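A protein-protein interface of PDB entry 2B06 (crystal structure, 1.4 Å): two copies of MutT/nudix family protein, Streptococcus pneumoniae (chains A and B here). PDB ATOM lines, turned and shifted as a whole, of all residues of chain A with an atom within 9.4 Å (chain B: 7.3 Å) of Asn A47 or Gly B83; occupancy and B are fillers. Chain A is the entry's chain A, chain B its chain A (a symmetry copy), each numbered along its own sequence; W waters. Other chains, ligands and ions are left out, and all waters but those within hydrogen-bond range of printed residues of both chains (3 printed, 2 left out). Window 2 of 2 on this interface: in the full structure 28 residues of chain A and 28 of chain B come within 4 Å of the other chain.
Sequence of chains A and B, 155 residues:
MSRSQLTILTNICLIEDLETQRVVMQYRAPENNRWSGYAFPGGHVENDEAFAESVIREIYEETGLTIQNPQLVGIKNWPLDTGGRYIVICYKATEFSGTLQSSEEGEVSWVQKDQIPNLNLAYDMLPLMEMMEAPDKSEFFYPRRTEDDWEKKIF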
ATOM      1  N   THR A   7      25.115 -29.725 -34.135  1.00  0.00           N
ATOM      2  CA  THR A   7      25.005 -30.666 -33.023  1.00  0.00           C
ATOM      3  C   THR A   7      23.535 -30.853 -32.664  1.00  0.00           C
ATOM      4  O   THR A   7      22.849 -29.905 -32.266  1.00  0.00           O
ATOM      5  CB  THR A   7      25.811 -30.212 -31.816  1.00  0.00           C
ATOM      6  OG1 THR A   7      27.188 -30.132 -32.199  1.00  0.00           O
ATOM      7  CG2 THR A   7      25.653 -31.204 -30.668  1.00  0.00           C
ATOM      8  N   LEU A   9      20.579 -32.542 -30.467  1.00  0.00           N
ATOM      9  CA  LEU A   9      20.331 -33.081 -29.141  1.00  0.00           C
ATOM     10  C   LEU A   9      18.973 -33.729 -29.067  1.00  0.00           C
ATOM     11  O   LEU A   9      17.946 -33.067 -29.259  1.00  0.00           O
ATOM     12  CB  LEU A   9      20.427 -31.967 -28.099  1.00  0.00           C
ATOM     13  CG  LEU A   9      21.762 -31.226 -28.049  1.00  0.00           C
ATOM     14  CD1 LEU A   9      21.651 -30.073 -27.071  1.00  0.00           C
ATOM     15  CD2 LEU A   9      22.858 -32.179 -27.613  1.00  0.00           C
ATOM     16  N   HIS A  44      13.372 -34.371 -29.500  1.00  0.00           N
ATOM     17  CA  HIS A  44      14.419 -33.359 -29.550  1.00  0.00           C
ATOM     18  C   HIS A  44      14.396 -32.437 -28.340  1.00  0.00           C
ATOM     19  O   HIS A  44      13.329 -32.064 -27.834  1.00  0.00           O
ATOM     20  CB  HIS A  44      14.254 -32.548 -30.837  1.00  0.00           C
ATOM     21  CG  HIS A  44      14.764 -33.247 -32.058  1.00  0.00           C
ATOM     22  ND1 HIS A  44      14.120 -34.316 -32.646  1.00  0.00           N
ATOM     23  CD2 HIS A  44      15.876 -33.030 -32.798  1.00  0.00           C
ATOM     24  CE1 HIS A  44      14.815 -34.729 -33.690  1.00  0.00           C
ATOM     25  NE2 HIS A  44      15.887 -33.966 -33.803  1.00  0.00           N
ATOM     26  N   VAL A  45      15.582 -32.058 -27.878  1.00  0.00           N
ATOM     27  CA  VAL A  45      15.708 -31.193 -26.710  1.00  0.00           C
ATOM     28  C   VAL A  45      15.476 -29.744 -27.128  1.00  0.00           C
ATOM     29  O   VAL A  45      16.133 -29.249 -28.046  1.00  0.00           O
ATOM     30  CB  VAL A  45      17.110 -31.367 -26.067  1.00  0.00           C
ATOM     31  CG1 VAL A  45      17.265 -30.471 -24.839  1.00  0.00           C
ATOM     32  CG2 VAL A  45      17.354 -32.839 -25.704  1.00  0.00           C
ATOM     33  N   GLU A  46      14.540 -29.073 -26.454  1.00  0.00           N
ATOM     34  CA  GLU A  46      14.254 -27.661 -26.712  1.00  0.00           C
ATOM     35  C   GLU A  46      15.335 -26.783 -26.089  1.00  0.00           C
ATOM     36  O   GLU A  46      15.976 -27.179 -25.115  1.00  0.00           O
ATOM     37  CB  GLU A  46      12.901 -27.292 -26.122  1.00  0.00           C
ATOM     38  CG  GLU A  46      11.729 -27.947 -26.815  1.00  0.00           C
ATOM     39  CD  GLU A  46      10.391 -27.594 -26.165  1.00  0.00           C
ATOM     40  OE1 GLU A  46      10.377 -26.953 -25.087  1.00  0.00           O
ATOM     41  OE2 GLU A  46       9.350 -27.972 -26.729  1.00  0.00           O
ATOM     42  N   ASN A  47      15.519 -25.587 -26.645  1.00  0.00           N
ATOM     43  CA  ASN A  47      16.624 -24.693 -26.266  1.00  0.00           C
ATOM     44  C   ASN A  47      16.747 -24.341 -24.768  1.00  0.00           C
ATOM     45  O   ASN A  47      17.851 -24.149 -24.257  1.00  0.00           O
ATOM     46  CB  ASN A  47      16.583 -23.406 -27.103  1.00  0.00           C
ATOM     47  CG  ASN A  47      16.888 -23.648 -28.583  1.00  0.00           C
ATOM     48  OD1 ASN A  47      17.211 -24.759 -28.997  1.00  0.00           O
ATOM     49  ND2 ASN A  47      16.783 -22.588 -29.383  1.00  0.00           N
ATOM     50  N   ASP A  48      15.628 -24.254 -24.067  1.00  0.00           N
ATOM     51  CA  ASP A  48      15.669 -23.779 -22.682  1.00  0.00           C
ATOM     52  C   ASP A  48      15.519 -24.875 -21.625  1.00  0.00           C
ATOM     53  O   ASP A  48      15.662 -24.610 -20.428  1.00  0.00           O
ATOM     54  CB  ASP A  48      14.626 -22.667 -22.462  1.00  0.00           C
ATOM     55  CG  ASP A  48      13.196 -23.106 -22.792  1.00  0.00           C
ATOM     56  OD1 ASP A  48      12.961 -24.254 -23.240  1.00  0.00           O
ATOM     57  OD2 ASP A  48      12.276 -22.277 -22.596  1.00  0.00           O
ATOM     58  N   GLU A  49      15.244 -26.097 -22.060  1.00  0.00           N
ATOM     59  CA  GLU A  49      14.854 -27.135 -21.115  1.00  0.00           C
ATOM     60  C   GLU A  49      16.031 -28.030 -20.743  1.00  0.00           C
ATOM     61  O   GLU A  49      16.979 -28.211 -21.524  1.00  0.00           O
ATOM     62  CB  GLU A  49      13.672 -27.948 -21.650  1.00  0.00           C
ATOM     63  CG  GLU A  49      14.017 -28.817 -22.823  1.00  0.00           C
ATOM     64  CD  GLU A  49      12.831 -29.610 -23.362  1.00  0.00           C
ATOM     65  OE1 GLU A  49      11.743 -29.643 -22.736  1.00  0.00           O
ATOM     66  OE2 GLU A  49      12.992 -30.231 -24.431  1.00  0.00           O
ATOM     67  N   ALA A  50      15.962 -28.591 -19.542  1.00  0.00           N
ATOM     68  CA  ALA A  50      16.951 -29.560 -19.106  1.00  0.00           C
ATOM     69  C   ALA A  50      16.816 -30.854 -19.894  1.00  0.00           C
ATOM     70  O   ALA A  50      15.761 -31.126 -20.475  1.00  0.00           O
ATOM     71  CB  ALA A  50      16.776 -29.842 -17.632  1.00  0.00           C
ATOM     72  N   PHE A  51      17.846 -31.687 -19.878  1.00  0.00           N
ATOM     73  CA  PHE A  51      17.731 -32.976 -20.546  1.00  0.00           C
ATOM     74  C   PHE A  51      16.623 -33.835 -19.916  1.00  0.00           C
ATOM     75  O   PHE A  51      15.830 -34.443 -20.636  1.00  0.00           O
ATOM     76  CB  PHE A  51      19.072 -33.716 -20.547  1.00  0.00           C
ATOM     77  CG  PHE A  51      20.097 -33.091 -21.441  1.00  0.00           C
ATOM     78  CD1 PHE A  51      19.857 -32.981 -22.807  1.00  0.00           C
ATOM     79  CD2 PHE A  51      21.323 -32.662 -20.944  1.00  0.00           C
ATOM     80  CE1 PHE A  51      20.799 -32.405 -23.653  1.00  0.00           C
ATOM     81  CE2 PHE A  51      22.271 -32.077 -21.792  1.00  0.00           C
ATOM     82  CZ  PHE A  51      22.016 -31.964 -23.143  1.00  0.00           C
ATOM     83  N   GLU A  53      13.989 -32.766 -18.217  1.00  0.00           N
ATOM     84  CA  GLU A  53      12.728 -32.114 -18.562  1.00  0.00           C
ATOM     85  C   GLU A  53      12.310 -32.516 -19.971  1.00  0.00           C
ATOM     86  O   GLU A  53      11.139 -32.778 -20.221  1.00  0.00           O
ATOM     87  CB  GLU A  53      12.866 -30.593 -18.456  1.00  0.00           C
ATOM     88  CG  GLU A  53      12.995 -30.109 -17.030  1.00  0.00           C
ATOM     89  CD  GLU A  53      13.400 -28.638 -16.912  1.00  0.00           C
ATOM     90  OE1 GLU A  53      13.684 -27.962 -17.932  1.00  0.00           O
ATOM     91  OE2 GLU A  53      13.438 -28.116 -15.765  1.00  0.00           O
ATOM     92  N   SER A  54      13.268 -32.557 -20.891  1.00  0.00           N
ATOM     93  CA  SER A  54      12.975 -32.900 -22.282  1.00  0.00           C
ATOM     94  C   SER A  54      12.448 -34.310 -22.447  1.00  0.00           C
ATOM     95  O   SER A  54      11.487 -34.532 -23.183  1.00  0.00           O
ATOM     96  CB  SER A  54      14.214 -32.690 -23.140  1.00  0.00           C
ATOM     97  OG  SER A  54      13.924 -32.951 -24.502  1.00  0.00           O
ATOM     98  N   ARG A  57       8.909 -34.564 -21.052  1.00  0.00           N
ATOM     99  CA  ARG A  57       7.962 -33.900 -21.929  1.00  0.00           C
ATOM    100  C   ARG A  57       7.722 -34.679 -23.224  1.00  0.00           C
ATOM    101  O   ARG A  57       6.574 -34.896 -23.614  1.00  0.00           O
ATOM    102  CB  ARG A  57       8.434 -32.482 -22.224  1.00  0.00           C
ATOM    103  CG  ARG A  57       7.537 -31.722 -23.179  1.00  0.00           C
ATOM    104  CD  ARG A  57       8.207 -30.441 -23.670  1.00  0.00           C
ATOM    105  NE  ARG A  57       9.518 -30.660 -24.288  1.00  0.00           N
ATOM    106  CZ  ARG A  57       9.694 -31.214 -25.486  1.00  0.00           C
ATOM    107  NH1 ARG A  57       8.655 -31.625 -26.220  1.00  0.00           N
ATOM    108  NH2 ARG A  57      10.930 -31.362 -25.954  1.00  0.00           N
ATOM    109  N   SER B   4      27.054 -17.591 -28.100  1.00  0.00           N
ATOM    110  CA  SER B   4      25.897 -17.993 -27.294  1.00  0.00           C
ATOM    111  C   SER B   4      24.906 -18.870 -28.068  1.00  0.00           C
ATOM    112  O   SER B   4      23.886 -19.295 -27.513  1.00  0.00           O
ATOM    113  CB  SER B   4      25.192 -16.762 -26.704  1.00  0.00           C
ATOM    114  OG  SER B   4      24.691 -15.913 -27.718  1.00  0.00           O
ATOM    115  N   GLN B   5      25.204 -19.117 -29.345  1.00  0.00           N
ATOM    116  CA  GLN B   5      24.417 -20.012 -30.200  1.00  0.00           C
ATOM    117  C   GLN B   5      25.037 -21.404 -30.299  1.00  0.00           C
ATOM    118  O   GLN B   5      24.401 -22.340 -30.782  1.00  0.00           O
ATOM    119  CB  GLN B   5      24.260 -19.417 -31.607  1.00  0.00           C
ATOM    120  CG  GLN B   5      23.504 -18.106 -31.638  1.00  0.00           C
ATOM    121  CD  GLN B   5      23.245 -17.602 -33.039  1.00  0.00           C
ATOM    122  OE1 GLN B   5      22.206 -17.893 -33.634  1.00  0.00           O
ATOM    123  NE2 GLN B   5      24.186 -16.837 -33.577  1.00  0.00           N
ATOM    124  N   LEU B   6      26.274 -21.543 -29.833  1.00  0.00           N
ATOM    125  CA  LEU B   6      27.029 -22.788 -30.003  1.00  0.00           C
ATOM    126  C   LEU B   6      26.679 -23.864 -28.984  1.00  0.00           C
ATOM    127  O   LEU B   6      26.272 -23.560 -27.860  1.00  0.00           O
ATOM    128  CB  LEU B   6      28.532 -22.501 -29.928  1.00  0.00           C
ATOM    129  CG  LEU B   6      29.132 -21.533 -30.945  1.00  0.00           C
ATOM    130  CD1 LEU B   6      30.536 -21.167 -30.492  1.00  0.00           C
ATOM    131  CD2 LEU B   6      29.134 -22.139 -32.352  1.00  0.00           C
ATOM    132  N   THR B   7      26.833 -25.127 -29.385  1.00  0.00           N
ATOM    133  CA  THR B   7      26.789 -26.246 -28.447  1.00  0.00           C
ATOM    134  C   THR B   7      28.211 -26.714 -28.154  1.00  0.00           C
ATOM    135  O   THR B   7      28.934 -27.161 -29.052  1.00  0.00           O
ATOM    136  CB  THR B   7      25.932 -27.389 -28.969  1.00  0.00           C
ATOM    137  OG1 THR B   7      24.597 -26.903 -29.148  1.00  0.00           O
ATOM    138  CG2 THR B   7      25.929 -28.547 -27.977  1.00  0.00           C
ATOM    139  N   TRP B  78      24.042 -26.231 -19.198  1.00  0.00           N
ATOM    140  CA  TRP B  78      23.229 -25.022 -19.061  1.00  0.00           C
ATOM    141  C   TRP B  78      23.031 -24.371 -20.412  1.00  0.00           C
ATOM    142  O   TRP B  78      23.900 -24.474 -21.278  1.00  0.00           O
ATOM    143  CB  TRP B  78      23.839 -24.046 -18.037  1.00  0.00           C
ATOM    144  CG  TRP B  78      25.238 -23.567 -18.342  1.00  0.00           C
ATOM    145  CD1 TRP B  78      25.584 -22.426 -19.008  1.00  0.00           C
ATOM    146  CD2 TRP B  78      26.469 -24.198 -17.969  1.00  0.00           C
ATOM    147  NE1 TRP B  78      26.953 -22.316 -19.085  1.00  0.00           N
ATOM    148  CE2 TRP B  78      27.523 -23.382 -18.444  1.00  0.00           C
ATOM    149  CE3 TRP B  78      26.785 -25.369 -17.273  1.00  0.00           C
ATOM    150  CZ2 TRP B  78      28.872 -23.711 -18.259  1.00  0.00           C
ATOM    151  CZ3 TRP B  78      28.128 -25.706 -17.096  1.00  0.00           C
ATOM    152  CH2 TRP B  78      29.154 -24.871 -17.582  1.00  0.00           C
ATOM    153  N   PRO B  79      21.866 -23.732 -20.614  1.00  0.00           N
ATOM    154  CA  PRO B  79      21.621 -23.038 -21.863  1.00  0.00           C
ATOM    155  C   PRO B  79      22.492 -21.808 -21.940  1.00  0.00           C
ATOM    156  O   PRO B  79      22.859 -21.216 -20.909  1.00  0.00           O
ATOM    157  CB  PRO B  79      20.138 -22.621 -21.766  1.00  0.00           C
ATOM    158  CG  PRO B  79      19.574 -23.378 -20.607  1.00  0.00           C
ATOM    159  CD  PRO B  79      20.728 -23.614 -19.690  1.00  0.00           C
ATOM    160  N   LEU B  80      22.837 -21.442 -23.167  1.00  0.00           N
ATOM    161  CA  LEU B  80      23.504 -20.187 -23.440  1.00  0.00           C
ATOM    162  C   LEU B  80      22.456 -19.208 -23.966  1.00  0.00           C
ATOM    163  O   LEU B  80      21.327 -19.608 -24.272  1.00  0.00           O
ATOM    164  CB  LEU B  80      24.657 -20.407 -24.424  1.00  0.00           C
ATOM    165  CG  LEU B  80      25.720 -21.414 -23.953  1.00  0.00           C
ATOM    166  CD1 LEU B  80      26.775 -21.626 -25.023  1.00  0.00           C
ATOM    167  CD2 LEU B  80      26.370 -20.990 -22.627  1.00  0.00           C
ATOM    168  N   ASP B  81      22.825 -17.932 -24.064  1.00  0.00           N
ATOM    169  CA  ASP B  81      21.859 -16.838 -24.273  1.00  0.00           C
ATOM    170  C   ASP B  81      21.017 -16.901 -25.546  1.00  0.00           C
ATOM    171  O   ASP B  81      19.906 -16.357 -25.582  1.00  0.00           O
ATOM    172  CB  ASP B  81      22.567 -15.479 -24.215  1.00  0.00           C
ATOM    173  CG  ASP B  81      23.032 -15.110 -22.814  1.00  0.00           C
ATOM    174  OD1 ASP B  81      22.624 -15.774 -21.838  1.00  0.00           O
ATOM    175  OD2 ASP B  81      23.810 -14.139 -22.690  1.00  0.00           O
ATOM    176  N   THR B  82      21.541 -17.540 -26.589  1.00  0.00           N
ATOM    177  CA  THR B  82      20.901 -17.494 -27.904  1.00  0.00           C
ATOM    178  C   THR B  82      20.772 -18.886 -28.532  1.00  0.00           C
ATOM    179  O   THR B  82      21.110 -19.096 -29.699  1.00  0.00           O
ATOM    180  CB  THR B  82      21.639 -16.514 -28.853  1.00  0.00           C
ATOM    181  OG1 THR B  82      22.107 -15.379 -28.109  1.00  0.00           O
ATOM    182  CG2 THR B  82      20.717 -16.027 -29.963  1.00  0.00           C
ATOM    183  N   GLY B  83      20.292 -19.842 -27.740  1.00  0.00           N
ATOM    184  CA  GLY B  83      19.957 -21.157 -28.262  1.00  0.00           C
ATOM    185  C   GLY B  83      21.070 -22.173 -28.101  1.00  0.00           C
ATOM    186  O   GLY B  83      20.882 -23.351 -28.396  1.00  0.00           O
ATOM    187  N   GLY B  84      22.237 -21.721 -27.641  1.00  0.00           N
ATOM    188  CA  GLY B  84      23.364 -22.621 -27.415  1.00  0.00           C
ATOM    189  C   GLY B  84      23.243 -23.389 -26.115  1.00  0.00           C
ATOM    190  O   GLY B  84      22.299 -23.194 -25.338  1.00  0.00           O
ATOM    191  N   ARG B  85      24.198 -24.271 -25.871  1.00  0.00           N
ATOM    192  CA  ARG B  85      24.213 -25.021 -24.628  1.00  0.00           C
ATOM    193  C   ARG B  85      25.634 -25.421 -24.313  1.00  0.00           C
ATOM    194  O   ARG B  85      26.375 -25.813 -25.210  1.00  0.00           O
ATOM    195  CB  ARG B  85      23.338 -26.282 -24.731  1.00  0.00           C
ATOM    196  CG  ARG B  85      23.110 -27.031 -23.391  1.00  0.00           C
ATOM    197  CD  ARG B  85      22.220 -28.251 -23.570  1.00  0.00           C
ATOM    198  NE  ARG B  85      20.875 -27.857 -24.010  1.00  0.00           N
ATOM    199  CZ  ARG B  85      19.779 -27.884 -23.245  1.00  0.00           C
ATOM    200  NH1 ARG B  85      19.822 -28.339 -21.996  1.00  0.00           N
ATOM    201  NH2 ARG B  85      18.626 -27.487 -23.752  1.00  0.00           N
ATOM    202  N   PHE B 141      21.790 -29.097 -13.753  1.00  0.00           N
ATOM    203  CA  PHE B 141      21.333 -28.149 -14.757  1.00  0.00           C
ATOM    204  C   PHE B 141      21.194 -26.760 -14.163  1.00  0.00           C
ATOM    205  O   PHE B 141      20.630 -26.613 -13.086  1.00  0.00           O
ATOM    206  CB  PHE B 141      19.974 -28.631 -15.274  1.00  0.00           C
ATOM    207  CG  PHE B 141      19.327 -27.735 -16.280  1.00  0.00           C
ATOM    208  CD1 PHE B 141      19.845 -27.587 -17.559  1.00  0.00           C
ATOM    209  CD2 PHE B 141      18.139 -27.078 -15.971  1.00  0.00           C
ATOM    210  CE1 PHE B 141      19.213 -26.784 -18.508  1.00  0.00           C
ATOM    211  CE2 PHE B 141      17.501 -26.279 -16.922  1.00  0.00           C
ATOM    212  CZ  PHE B 141      18.037 -26.129 -18.183  1.00  0.00           C
ATOM    213  N   PRO B 143      19.110 -23.569 -14.990  1.00  0.00           N
ATOM    214  CA  PRO B 143      18.082 -23.069 -15.913  1.00  0.00           C
ATOM    215  C   PRO B 143      18.387 -21.707 -16.532  1.00  0.00           C
ATOM    216  O   PRO B 143      17.860 -21.403 -17.607  1.00  0.00           O
ATOM    217  CB  PRO B 143      16.813 -23.005 -15.053  1.00  0.00           C
ATOM    218  CG  PRO B 143      17.097 -23.843 -13.853  1.00  0.00           C
ATOM    219  CD  PRO B 143      18.570 -23.801 -13.638  1.00  0.00           C
HETATM  220  O   HOH W   1      22.700 -28.474 -30.085  1.00  0.00           O
HETATM  221  O   HOH W   2      15.991 -22.127 -19.310  1.00  0.00           O
HETATM  222  O   HOH W   3      29.027 -29.343 -30.485  1.00  0.00           O
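The backbone carbonyl oxygen (O) of Glu A49 lies within hydrogen-bond range of the guanidinium group (NH2) of Arg B85.
The guanidinium group of Arg B85 sits at hydrogen-bond distance from the backbone carbonyl oxygen of Glu A46, 3.0 Å away.
The backbone carbonyl oxygen of Asn A47 sits at hydrogen-bond distance from the guanidinium group of Arg B85.
The guanidinium group (NH2) of Arg A57 is in salt-bridge range of the side-chain carboxylate (OE2) of Glu A49 (2.8 Å).
The side-chain carboxylate of Glu A49 is in hydrogen-bond range of the side-chain hydroxyl of Ser A54.
N of Ala A50 is in hydrogen-bond range of OE1 of Glu A53, 2.9 Å away.
N of Arg B85 sits at hydrogen-bond distance from O of Leu B6.
N of Glu A46 lies within hydrogen-bond range of OE2 of Glu A49 (2.8 Å).
OE2 of Glu A46 is in salt-bridge range of NE of Arg A57 (3.6 Å).
Among the printed residues, merely in contact across the chains: Thr A7 with Thr B7 (3.8 Å), Leu A9 with Arg B85 (3.9 Å), Val A45 with Arg B85 (3.5 Å), Asn A47 with Pro B79 (3.7 Å), Asn A47 with Gly B83 (3.7 Å), Asp A48 with Phe B141 (3.6 Å), Glu A49 with Phe B141 (3.8 Å), Ala A50 with Phe B141 (3.5 Å) and Phe A51 with Arg B85 (3.7 Å).
Of the printed residues of chain B, Asn A47 touches Pro B79, Gly B83 and Arg B85.
Gly B83 touches one residue of chain A.
No residue of chain A comes within 4 Å of Thr B82.
Gly B84 touches none of the printed residues of chain A.
Printed residues of chain B within 4 Å of Ala A50: Phe B141 (3.5 Å).
Of the printed residues of chain B, Glu A49 touches Arg B85 and Phe B141.
Of the printed residues of chain B, Val A45 touches Arg B85.
Pro B143 touches none of the printed residues of chain A.
Gln B5 touches none of the printed residues of chain A.
Printed residues of chain A that touch a printed residue of chain B: Thr A7, Leu A9, Val A45, Glu A46, Asn A47, Asp A48, Glu A49, Ala A50 and Phe A51.
Hydrophobic or aromatic side chains of chain A that line the printed part of chain B: Leu A9, Val A45, Ala A50 and Phe A51.
Among the printed residues, no Asp or Glu carboxylate lies within 4 Å of a Lys or Arg side-chain nitrogen of the other chain.
Thr A7 touches its own counterpart, Thr B7.
Of the 12 pairs that touch across the chains among the printed residues, 1 has its exchanged pair printed and touching as well.
Water W1 lies within hydrogen-bond range of O of Thr A7 (2.6 Å) and OG1 of Thr B7 (2.6 Å).
Water W3 bridges O of Thr B7 (2.6 Å) and OG1 of Thr A7 (2.6 Å).
Water W2 lies within hydrogen-bond range of the backbone carbonyl oxygen of Pro B143 and the backbone carbonyl oxygen of Asp A48.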
